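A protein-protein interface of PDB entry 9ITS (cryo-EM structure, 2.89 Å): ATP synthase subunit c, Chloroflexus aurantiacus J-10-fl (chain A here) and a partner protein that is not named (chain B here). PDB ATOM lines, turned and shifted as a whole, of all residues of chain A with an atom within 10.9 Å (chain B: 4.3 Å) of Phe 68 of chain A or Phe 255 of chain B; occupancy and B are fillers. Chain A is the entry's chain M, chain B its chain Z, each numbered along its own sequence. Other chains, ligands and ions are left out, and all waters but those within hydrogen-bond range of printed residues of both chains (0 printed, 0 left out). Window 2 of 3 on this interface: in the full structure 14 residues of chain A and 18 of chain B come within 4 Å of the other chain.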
ATOM      1  N   ASN A   5     -17.694   6.206  -1.802  1.00  0.00           N
ATOM      2  CA  ASN A   5     -16.801   6.414  -0.668  1.00  0.00           C
ATOM      3  C   ASN A   5     -16.024   7.717  -0.797  1.00  0.00           C
ATOM      4  O   ASN A   5     -15.756   8.379   0.212  1.00  0.00           O
ATOM      5  CB  ASN A   5     -15.841   5.233  -0.534  1.00  0.00           C
ATOM      6  CG  ASN A   5     -15.124   4.915  -1.831  1.00  0.00           C
ATOM      7  OD1 ASN A   5     -15.495   5.413  -2.895  1.00  0.00           O
ATOM      8  ND2 ASN A   5     -14.093   4.083  -1.749  1.00  0.00           N
ATOM      9  N   LEU A   6     -15.650   8.096  -2.022  1.00  0.00           N
ATOM     10  CA  LEU A   6     -14.985   9.380  -2.230  1.00  0.00           C
ATOM     11  C   LEU A   6     -15.900  10.538  -1.853  1.00  0.00           C
ATOM     12  O   LEU A   6     -15.462  11.508  -1.224  1.00  0.00           O
ATOM     13  CB  LEU A   6     -14.535   9.504  -3.685  1.00  0.00           C
ATOM     14  CG  LEU A   6     -13.622   8.396  -4.211  1.00  0.00           C
ATOM     15  CD1 LEU A   6     -13.361   8.580  -5.699  1.00  0.00           C
ATOM     16  CD2 LEU A   6     -12.317   8.364  -3.433  1.00  0.00           C
ATOM     17  N   ALA A   8     -18.351  10.365   0.299  1.00  0.00           N
ATOM     18  CA  ALA A   8     -18.453  10.322   1.755  1.00  0.00           C
ATOM     19  C   ALA A   8     -17.258  11.003   2.411  1.00  0.00           C
ATOM     20  O   ALA A   8     -17.415  11.821   3.327  1.00  0.00           O
ATOM     21  CB  ALA A   8     -18.567   8.873   2.224  1.00  0.00           C
ATOM     22  N   THR A   9     -16.050  10.674   1.945  1.00  0.00           N
ATOM     23  CA  THR A   9     -14.841  11.295   2.476  1.00  0.00           C
ATOM     24  C   THR A   9     -14.877  12.805   2.292  1.00  0.00           C
ATOM     25  O   THR A   9     -14.566  13.564   3.222  1.00  0.00           O
ATOM     26  CB  THR A   9     -13.611  10.703   1.785  1.00  0.00           C
ATOM     27  OG1 THR A   9     -13.762   9.282   1.670  1.00  0.00           O
ATOM     28  CG2 THR A   9     -12.347  11.016   2.562  1.00  0.00           C
ATOM     29  N   ALA A  10     -15.275  13.257   1.101  1.00  0.00           N
ATOM     30  CA  ALA A  10     -15.346  14.686   0.823  1.00  0.00           C
ATOM     31  C   ALA A  10     -16.338  15.380   1.743  1.00  0.00           C
ATOM     32  O   ALA A  10     -16.045  16.444   2.297  1.00  0.00           O
ATOM     33  CB  ALA A  10     -15.726  14.908  -0.636  1.00  0.00           C
ATOM     34  N   LEU A  11     -17.521  14.784   1.925  1.00  0.00           N
ATOM     35  CA  LEU A  11     -18.534  15.389   2.785  1.00  0.00           C
ATOM     36  C   LEU A  11     -18.053  15.482   4.225  1.00  0.00           C
ATOM     37  O   LEU A  11     -18.206  16.528   4.873  1.00  0.00           O
ATOM     38  CB  LEU A  11     -19.833  14.585   2.709  1.00  0.00           C
ATOM     39  CG  LEU A  11     -20.671  14.716   1.436  1.00  0.00           C
ATOM     40  CD1 LEU A  11     -21.800  13.698   1.439  1.00  0.00           C
ATOM     41  CD2 LEU A  11     -21.219  16.124   1.290  1.00  0.00           C
ATOM     42  N   ALA A  12     -17.457  14.403   4.741  1.00  0.00           N
ATOM     43  CA  ALA A  12     -16.998  14.402   6.126  1.00  0.00           C
ATOM     44  C   ALA A  12     -15.908  15.443   6.347  1.00  0.00           C
ATOM     45  O   ALA A  12     -15.973  16.233   7.303  1.00  0.00           O
ATOM     46  CB  ALA A  12     -16.499  13.009   6.512  1.00  0.00           C
ATOM     47  N   VAL A  13     -14.910  15.480   5.459  1.00  0.00           N
ATOM     48  CA  VAL A  13     -13.814  16.428   5.626  1.00  0.00           C
ATOM     49  C   VAL A  13     -14.309  17.858   5.447  1.00  0.00           C
ATOM     50  O   VAL A  13     -13.875  18.770   6.159  1.00  0.00           O
ATOM     51  CB  VAL A  13     -12.661  16.093   4.664  1.00  0.00           C
ATOM     52  CG1 VAL A  13     -11.526  17.079   4.836  1.00  0.00           C
ATOM     53  CG2 VAL A  13     -12.160  14.690   4.926  1.00  0.00           C
ATOM     54  N   GLY A  14     -15.244  18.078   4.521  1.00  0.00           N
ATOM     55  CA  GLY A  14     -15.774  19.416   4.326  1.00  0.00           C
ATOM     56  C   GLY A  14     -16.544  19.929   5.526  1.00  0.00           C
ATOM     57  O   GLY A  14     -16.366  21.076   5.940  1.00  0.00           O
ATOM     58  N   GLU A  57     -10.262  21.348  17.092  1.00  0.00           N
ATOM     59  CA  GLU A  57      -9.443  20.459  16.280  1.00  0.00           C
ATOM     60  C   GLU A  57      -9.750  19.000  16.575  1.00  0.00           C
ATOM     61  O   GLU A  57      -9.596  18.154  15.697  1.00  0.00           O
ATOM     62  CB  GLU A  57      -7.957  20.741  16.504  1.00  0.00           C
ATOM     63  CG  GLU A  57      -7.063  20.150  15.423  1.00  0.00           C
ATOM     64  CD  GLU A  57      -5.651  20.695  15.463  1.00  0.00           C
ATOM     65  OE1 GLU A  57      -5.011  20.611  16.531  1.00  0.00           O
ATOM     66  OE2 GLU A  57      -5.178  21.201  14.423  1.00  0.00           O
ATOM     67  N   ALA A  60     -12.708  18.291  14.375  1.00  0.00           N
ATOM     68  CA  ALA A  60     -12.266  18.230  12.983  1.00  0.00           C
ATOM     69  C   ALA A  60     -11.480  16.951  12.709  1.00  0.00           C
ATOM     70  O   ALA A  60     -11.628  16.325  11.652  1.00  0.00           O
ATOM     71  CB  ALA A  60     -11.425  19.461  12.645  1.00  0.00           C
ATOM     72  N   ILE A  61     -10.641  16.544  13.661  1.00  0.00           N
ATOM     73  CA  ILE A  61      -9.840  15.339  13.505  1.00  0.00           C
ATOM     74  C   ILE A  61     -10.701  14.092  13.653  1.00  0.00           C
ATOM     75  O   ILE A  61     -10.408  13.061  13.048  1.00  0.00           O
ATOM     76  CB  ILE A  61      -8.657  15.378  14.497  1.00  0.00           C
ATOM     77  CG1 ILE A  61      -7.608  16.384  14.018  1.00  0.00           C
ATOM     78  CG2 ILE A  61      -8.003  14.030  14.647  1.00  0.00           C
ATOM     79  CD1 ILE A  61      -7.063  16.089  12.638  1.00  0.00           C
ATOM     80  N   PHE A  62     -11.787  14.162  14.429  1.00  0.00           N
ATOM     81  CA  PHE A  62     -12.783  13.093  14.392  1.00  0.00           C
ATOM     82  C   PHE A  62     -13.313  12.911  12.980  1.00  0.00           C
ATOM     83  O   PHE A  62     -13.381  11.787  12.462  1.00  0.00           O
ATOM     84  CB  PHE A  62     -13.948  13.396  15.339  1.00  0.00           C
ATOM     85  CG  PHE A  62     -13.592  13.349  16.792  1.00  0.00           C
ATOM     86  CD1 PHE A  62     -12.413  12.765  17.222  1.00  0.00           C
ATOM     87  CD2 PHE A  62     -14.452  13.887  17.735  1.00  0.00           C
ATOM     88  CE1 PHE A  62     -12.099  12.725  18.562  1.00  0.00           C
ATOM     89  CE2 PHE A  62     -14.142  13.848  19.075  1.00  0.00           C
ATOM     90  CZ  PHE A  62     -12.967  13.267  19.486  1.00  0.00           C
ATOM     91  N   GLY A  63     -13.688  14.021  12.343  1.00  0.00           N
ATOM     92  CA  GLY A  63     -14.146  13.948  10.962  1.00  0.00           C
ATOM     93  C   GLY A  63     -13.100  13.356  10.034  1.00  0.00           C
ATOM     94  O   GLY A  63     -13.393  12.473   9.222  1.00  0.00           O
ATOM     95  N   LEU A  64     -11.853  13.810  10.175  1.00  0.00           N
ATOM     96  CA  LEU A  64     -10.786  13.347   9.291  1.00  0.00           C
ATOM     97  C   LEU A  64     -10.446  11.878   9.536  1.00  0.00           C
ATOM     98  O   LEU A  64     -10.135  11.140   8.596  1.00  0.00           O
ATOM     99  CB  LEU A  64      -9.551  14.228   9.471  1.00  0.00           C
ATOM    100  CG  LEU A  64      -8.491  14.171   8.372  1.00  0.00           C
ATOM    101  CD1 LEU A  64      -9.125  14.342   7.004  1.00  0.00           C
ATOM    102  CD2 LEU A  64      -7.448  15.247   8.610  1.00  0.00           C
ATOM    103  N   VAL A  65     -10.506  11.434  10.793  1.00  0.00           N
ATOM    104  CA  VAL A  65     -10.189  10.047  11.126  1.00  0.00           C
ATOM    105  C   VAL A  65     -11.277   9.116  10.610  1.00  0.00           C
ATOM    106  O   VAL A  65     -10.994   8.029  10.092  1.00  0.00           O
ATOM    107  CB  VAL A  65      -9.979   9.899  12.645  1.00  0.00           C
ATOM    108  CG1 VAL A  65     -10.156   8.453  13.091  1.00  0.00           C
ATOM    109  CG2 VAL A  65      -8.598  10.404  13.037  1.00  0.00           C
ATOM    110  N   ILE A  66     -12.542   9.525  10.743  1.00  0.00           N
ATOM    111  CA  ILE A  66     -13.615   8.724  10.165  1.00  0.00           C
ATOM    112  C   ILE A  66     -13.502   8.701   8.645  1.00  0.00           C
ATOM    113  O   ILE A  66     -13.778   7.675   8.010  1.00  0.00           O
ATOM    114  CB  ILE A  66     -14.984   9.241  10.642  1.00  0.00           C
ATOM    115  CG1 ILE A  66     -15.094   9.083  12.159  1.00  0.00           C
ATOM    116  CG2 ILE A  66     -16.117   8.496   9.954  1.00  0.00           C
ATOM    117  CD1 ILE A  66     -15.110   7.642  12.624  1.00  0.00           C
ATOM    118  N   ALA A  67     -13.068   9.810   8.040  1.00  0.00           N
ATOM    119  CA  ALA A  67     -12.809   9.815   6.604  1.00  0.00           C
ATOM    120  C   ALA A  67     -11.705   8.830   6.231  1.00  0.00           C
ATOM    121  O   ALA A  67     -11.805   8.128   5.217  1.00  0.00           O
ATOM    122  CB  ALA A  67     -12.444  11.227   6.150  1.00  0.00           C
ATOM    123  N   PHE A  68     -10.640   8.775   7.033  1.00  0.00           N
ATOM    124  CA  PHE A  68      -9.556   7.828   6.777  1.00  0.00           C
ATOM    125  C   PHE A  68     -10.029   6.385   6.921  1.00  0.00           C
ATOM    126  O   PHE A  68      -9.643   5.519   6.129  1.00  0.00           O
ATOM    127  CB  PHE A  68      -8.384   8.099   7.719  1.00  0.00           C
ATOM    128  CG  PHE A  68      -7.618   9.347   7.390  1.00  0.00           C
ATOM    129  CD1 PHE A  68      -7.407   9.721   6.074  1.00  0.00           C
ATOM    130  CD2 PHE A  68      -7.096  10.140   8.399  1.00  0.00           C
ATOM    131  CE1 PHE A  68      -6.701  10.867   5.768  1.00  0.00           C
ATOM    132  CE2 PHE A  68      -6.386  11.287   8.100  1.00  0.00           C
ATOM    133  CZ  PHE A  68      -6.188  11.651   6.783  1.00  0.00           C
ATOM    134  N   LEU A  69     -10.854   6.110   7.934  1.00  0.00           N
ATOM    135  CA  LEU A  69     -11.438   4.782   8.093  1.00  0.00           C
ATOM    136  C   LEU A  69     -12.330   4.409   6.917  1.00  0.00           C
ATOM    137  O   LEU A  69     -12.336   3.246   6.501  1.00  0.00           O
ATOM    138  CB  LEU A  69     -12.245   4.704   9.391  1.00  0.00           C
ATOM    139  CG  LEU A  69     -11.489   4.842  10.713  1.00  0.00           C
ATOM    140  CD1 LEU A  69     -12.463   4.869  11.880  1.00  0.00           C
ATOM    141  CD2 LEU A  69     -10.484   3.714  10.877  1.00  0.00           C
ATOM    142  N   ILE A  70     -13.087   5.365   6.390  1.00  0.00           N
ATOM    143  CA  ILE A  70     -13.895   5.135   5.201  1.00  0.00           C
ATOM    144  C   ILE A  70     -13.037   4.853   3.968  1.00  0.00           C
ATOM    145  O   ILE A  70     -13.341   3.931   3.204  1.00  0.00           O
ATOM    146  CB  ILE A  70     -14.823   6.342   4.979  1.00  0.00           C
ATOM    147  CG1 ILE A  70     -16.003   6.278   5.949  1.00  0.00           C
ATOM    148  CG2 ILE A  70     -15.297   6.425   3.534  1.00  0.00           C
ATOM    149  CD1 ILE A  70     -16.607   7.619   6.258  1.00  0.00           C
ATOM    150  N   GLY A  71     -11.959   5.616   3.770  1.00  0.00           N
ATOM    151  CA  GLY A  71     -11.145   5.442   2.579  1.00  0.00           C
ATOM    152  C   GLY A  71     -10.399   4.124   2.534  1.00  0.00           C
ATOM    153  O   GLY A  71     -10.084   3.625   1.449  1.00  0.00           O
ATOM    154  N   PHE A  72     -10.108   3.541   3.693  1.00  0.00           N
ATOM    155  CA  PHE A  72      -9.366   2.286   3.749  1.00  0.00           C
ATOM    156  C   PHE A  72     -10.071   1.259   4.630  1.00  0.00           C
ATOM    157  O   PHE A  72     -11.297   1.254   4.742  1.00  0.00           O
ATOM    158  CB  PHE A  72      -7.945   2.527   4.259  1.00  0.00           C
ATOM    159  CG  PHE A  72      -7.292   3.746   3.673  1.00  0.00           C
ATOM    160  CD1 PHE A  72      -6.950   3.788   2.332  1.00  0.00           C
ATOM    161  CD2 PHE A  72      -7.025   4.853   4.462  1.00  0.00           C
ATOM    162  CE1 PHE A  72      -6.353   4.910   1.788  1.00  0.00           C
ATOM    163  CE2 PHE A  72      -6.427   5.978   3.924  1.00  0.00           C
ATOM    164  CZ  PHE A  72      -6.092   6.006   2.585  1.00  0.00           C
ATOM    165  N   VAL B  34      -0.734   3.705   4.450  1.00  0.00           N
ATOM    166  CA  VAL B  34      -1.003   2.680   5.453  1.00  0.00           C
ATOM    167  C   VAL B  34      -1.449   3.350   6.745  1.00  0.00           C
ATOM    168  O   VAL B  34      -0.784   4.261   7.251  1.00  0.00           O
ATOM    169  CB  VAL B  34       0.238   1.804   5.681  1.00  0.00           C
ATOM    170  CG1 VAL B  34      -0.050   0.733   6.722  1.00  0.00           C
ATOM    171  CG2 VAL B  34       0.692   1.176   4.372  1.00  0.00           C
ATOM    172  N   ALA B  35      -2.579   2.895   7.284  1.00  0.00           N
ATOM    173  CA  ALA B  35      -3.127   3.420   8.525  1.00  0.00           C
ATOM    174  C   ALA B  35      -2.791   2.549   9.727  1.00  0.00           C
ATOM    175  O   ALA B  35      -3.378   2.734  10.798  1.00  0.00           O
ATOM    176  CB  ALA B  35      -4.643   3.586   8.405  1.00  0.00           C
ATOM    177  N   ARG B 185       8.395   5.352  10.916  1.00  0.00           N
ATOM    178  CA  ARG B 185       7.061   5.930  11.011  1.00  0.00           C
ATOM    179  C   ARG B 185       6.872   6.555  12.388  1.00  0.00           C
ATOM    180  O   ARG B 185       7.205   5.938  13.403  1.00  0.00           O
ATOM    181  CB  ARG B 185       6.001   4.858  10.763  1.00  0.00           C
ATOM    182  CG  ARG B 185       4.583   5.279  11.103  1.00  0.00           C
ATOM    183  CD  ARG B 185       3.646   4.083  11.090  1.00  0.00           C
ATOM    184  NE  ARG B 185       2.248   4.477  10.975  1.00  0.00           N
ATOM    185  CZ  ARG B 185       1.647   4.786   9.834  1.00  0.00           C
ATOM    186  NH1 ARG B 185       2.296   4.760   8.682  1.00  0.00           N
ATOM    187  NH2 ARG B 185       0.362   5.127   9.850  1.00  0.00           N
ATOM    188  N   PHE B 251      -3.315  11.241  16.864  1.00  0.00           N
ATOM    189  CA  PHE B 251      -3.175  10.301  15.756  1.00  0.00           C
ATOM    190  C   PHE B 251      -3.580  10.945  14.437  1.00  0.00           C
ATOM    191  O   PHE B 251      -2.842  10.878  13.446  1.00  0.00           O
ATOM    192  CB  PHE B 251      -4.009   9.047  16.025  1.00  0.00           C
ATOM    193  CG  PHE B 251      -4.466   8.342  14.778  1.00  0.00           C
ATOM    194  CD1 PHE B 251      -3.566   7.640  13.995  1.00  0.00           C
ATOM    195  CD2 PHE B 251      -5.796   8.379  14.393  1.00  0.00           C
ATOM    196  CE1 PHE B 251      -3.982   6.992  12.848  1.00  0.00           C
ATOM    197  CE2 PHE B 251      -6.218   7.731  13.247  1.00  0.00           C
ATOM    198  CZ  PHE B 251      -5.310   7.037  12.474  1.00  0.00           C
ATOM    199  N   GLY B 252      -4.747  11.590  14.414  1.00  0.00           N
ATOM    200  CA  GLY B 252      -5.212  12.223  13.195  1.00  0.00           C
ATOM    201  C   GLY B 252      -4.351  13.394  12.774  1.00  0.00           C
ATOM    202  O   GLY B 252      -4.101  13.583  11.583  1.00  0.00           O
ATOM    203  N   ASN B 253      -3.876  14.192  13.737  1.00  0.00           N
ATOM    204  CA  ASN B 253      -3.025  15.326  13.393  1.00  0.00           C
ATOM    205  C   ASN B 253      -1.730  14.862  12.740  1.00  0.00           C
ATOM    206  O   ASN B 253      -1.324  15.389  11.697  1.00  0.00           O
ATOM    207  CB  ASN B 253      -2.731  16.159  14.639  1.00  0.00           C
ATOM    208  CG  ASN B 253      -3.814  17.178  14.927  1.00  0.00           C
ATOM    209  OD1 ASN B 253      -3.802  18.282  14.385  1.00  0.00           O
ATOM    210  ND2 ASN B 253      -4.756  16.812  15.788  1.00  0.00           N
ATOM    211  N   ILE B 254      -1.086  13.848  13.318  1.00  0.00           N
ATOM    212  CA  ILE B 254       0.183  13.386  12.762  1.00  0.00           C
ATOM    213  C   ILE B 254      -0.026  12.666  11.432  1.00  0.00           C
ATOM    214  O   ILE B 254       0.767  12.832  10.494  1.00  0.00           O
ATOM    215  CB  ILE B 254       0.920  12.510  13.789  1.00  0.00           C
ATOM    216  CG1 ILE B 254       1.200  13.330  15.050  1.00  0.00           C
ATOM    217  CG2 ILE B 254       2.220  11.972  13.213  1.00  0.00           C
ATOM    218  CD1 ILE B 254       1.777  14.707  14.771  1.00  0.00           C
ATOM    219  N   PHE B 255      -1.091  11.865  11.319  1.00  0.00           N
ATOM    220  CA  PHE B 255      -1.380  11.200  10.053  1.00  0.00           C
ATOM    221  C   PHE B 255      -1.678  12.211   8.953  1.00  0.00           C
ATOM    222  O   PHE B 255      -1.188  12.075   7.824  1.00  0.00           O
ATOM    223  CB  PHE B 255      -2.549  10.233  10.230  1.00  0.00           C
ATOM    224  CG  PHE B 255      -2.574   9.120   9.224  1.00  0.00           C
ATOM    225  CD1 PHE B 255      -3.135   9.311   7.973  1.00  0.00           C
ATOM    226  CD2 PHE B 255      -2.030   7.885   9.527  1.00  0.00           C
ATOM    227  CE1 PHE B 255      -3.160   8.289   7.045  1.00  0.00           C
ATOM    228  CE2 PHE B 255      -2.050   6.860   8.603  1.00  0.00           C
ATOM    229  CZ  PHE B 255      -2.614   7.062   7.361  1.00  0.00           C
ATOM    230  N   ALA B 256      -2.473  13.236   9.267  1.00  0.00           N
ATOM    231  CA  ALA B 256      -2.763  14.280   8.295  1.00  0.00           C
ATOM    232  C   ALA B 256      -1.498  15.026   7.905  1.00  0.00           C
ATOM    233  O   ALA B 256      -1.301  15.350   6.731  1.00  0.00           O
ATOM    234  CB  ALA B 256      -3.805  15.244   8.859  1.00  0.00           C
ATOM    235  N   GLY B 257      -0.619  15.288   8.874  1.00  0.00           N
ATOM    236  CA  GLY B 257       0.632  15.955   8.556  1.00  0.00           C
ATOM    237  C   GLY B 257       1.498  15.151   7.606  1.00  0.00           C
ATOM    238  O   GLY B 257       1.997  15.676   6.609  1.00  0.00           O
ATOM    239  N   GLU B 258       1.666  13.856   7.889  1.00  0.00           N
ATOM    240  CA  GLU B 258       2.546  13.047   7.048  1.00  0.00           C
ATOM    241  C   GLU B 258       1.953  12.835   5.657  1.00  0.00           C
ATOM    242  O   GLU B 258       2.682  12.878   4.655  1.00  0.00           O
ATOM    243  CB  GLU B 258       2.868  11.711   7.724  1.00  0.00           C
ATOM    244  CG  GLU B 258       1.678  10.832   8.047  1.00  0.00           C
ATOM    245  CD  GLU B 258       2.008   9.747   9.052  1.00  0.00           C
ATOM    246  OE1 GLU B 258       3.180   9.665   9.475  1.00  0.00           O
ATOM    247  OE2 GLU B 258       1.096   8.977   9.418  1.00  0.00           O
ATOM    248  N   VAL B 259       0.633  12.630   5.560  1.00  0.00           N
ATOM    249  CA  VAL B 259       0.052  12.494   4.228  1.00  0.00           C
ATOM    250  C   VAL B 259       0.085  13.827   3.490  1.00  0.00           C
ATOM    251  O   VAL B 259       0.196  13.853   2.262  1.00  0.00           O
ATOM    252  CB  VAL B 259      -1.372  11.902   4.282  1.00  0.00           C
ATOM    253  CG1 VAL B 259      -1.361  10.559   4.993  1.00  0.00           C
ATOM    254  CG2 VAL B 259      -2.354  12.863   4.932  1.00  0.00           C
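Phe 68 of chain A touches just one residue of chain B: Phe 255.
Of chain A, only Ile 61 and Val 65 come within 4 Å of Gly 252 of chain B.
No residue of chain A comes within 4 Å of Ile 254 of chain B.
No residue of chain A comes within 4 Å of Gly 257 of chain B.
No residue of chain A comes within 4 Å of Glu 258 of chain B.
Val 259 of chain B touches none of the printed residues of chain A.
Printed residues of chain B within 4 Å of Val 65 of chain A: Phe 251 (3.6 Å) and Gly 252 (3.8 Å).
Printed residues of chain B within 4 Å of Ile 61 of chain A: Gly 252 and Asn 253.
Printed residues of chain A within 4 Å of Asn 253 of chain B: Glu 57 and Ile 61.
Printed residues of chain B within 4 Å of Glu 57 of chain A: Asn 253.
Of the printed residues of chain B, Leu 64 of chain A touches Ala 256 (3.7 Å).
Ala 60 of chain A touches none of the printed residues of chain B.
The nearest residue of chain A that does not touch Phe 255 of chain B is Phe 72 of chain A (5.1 Å).
Of the 23 printed residues of chain A, 5 touch a printed residue of chain B.
Hydrophobic or aromatic side chains of chain A within 4 Å of the printed part of chain B: Ile 61, Leu 64, Val 65 and Phe 68.
Along chain A the printed residues that touch a printed residue of chain B span positions 57 to 68.
Hydrophobic or aromatic side chains of chain B within 4 Å of the printed part of chain A: Phe 251, Phe 255 and Ala 256.
OE2 of Glu 57 of chain A lies close to OD1 of Asn 253 of chain B (3.2 Å).
CG2 of Ile 61 of chain A touches CA of Gly 252 of chain B (3.6 Å).
Asn 253 of chain B touches Ile 61 of chain A.
Leu 64 of chain A touches Ala 256 of chain B.
Phe 251 of chain B touches Val 65 of chain A.
Gly 252 of chain B touches Val 65 of chain A (CA to CG2, 3.8 Å).
Phe 68 of chain A touches Phe 255 of chain B (CE2 to CD1, 3.8 Å).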
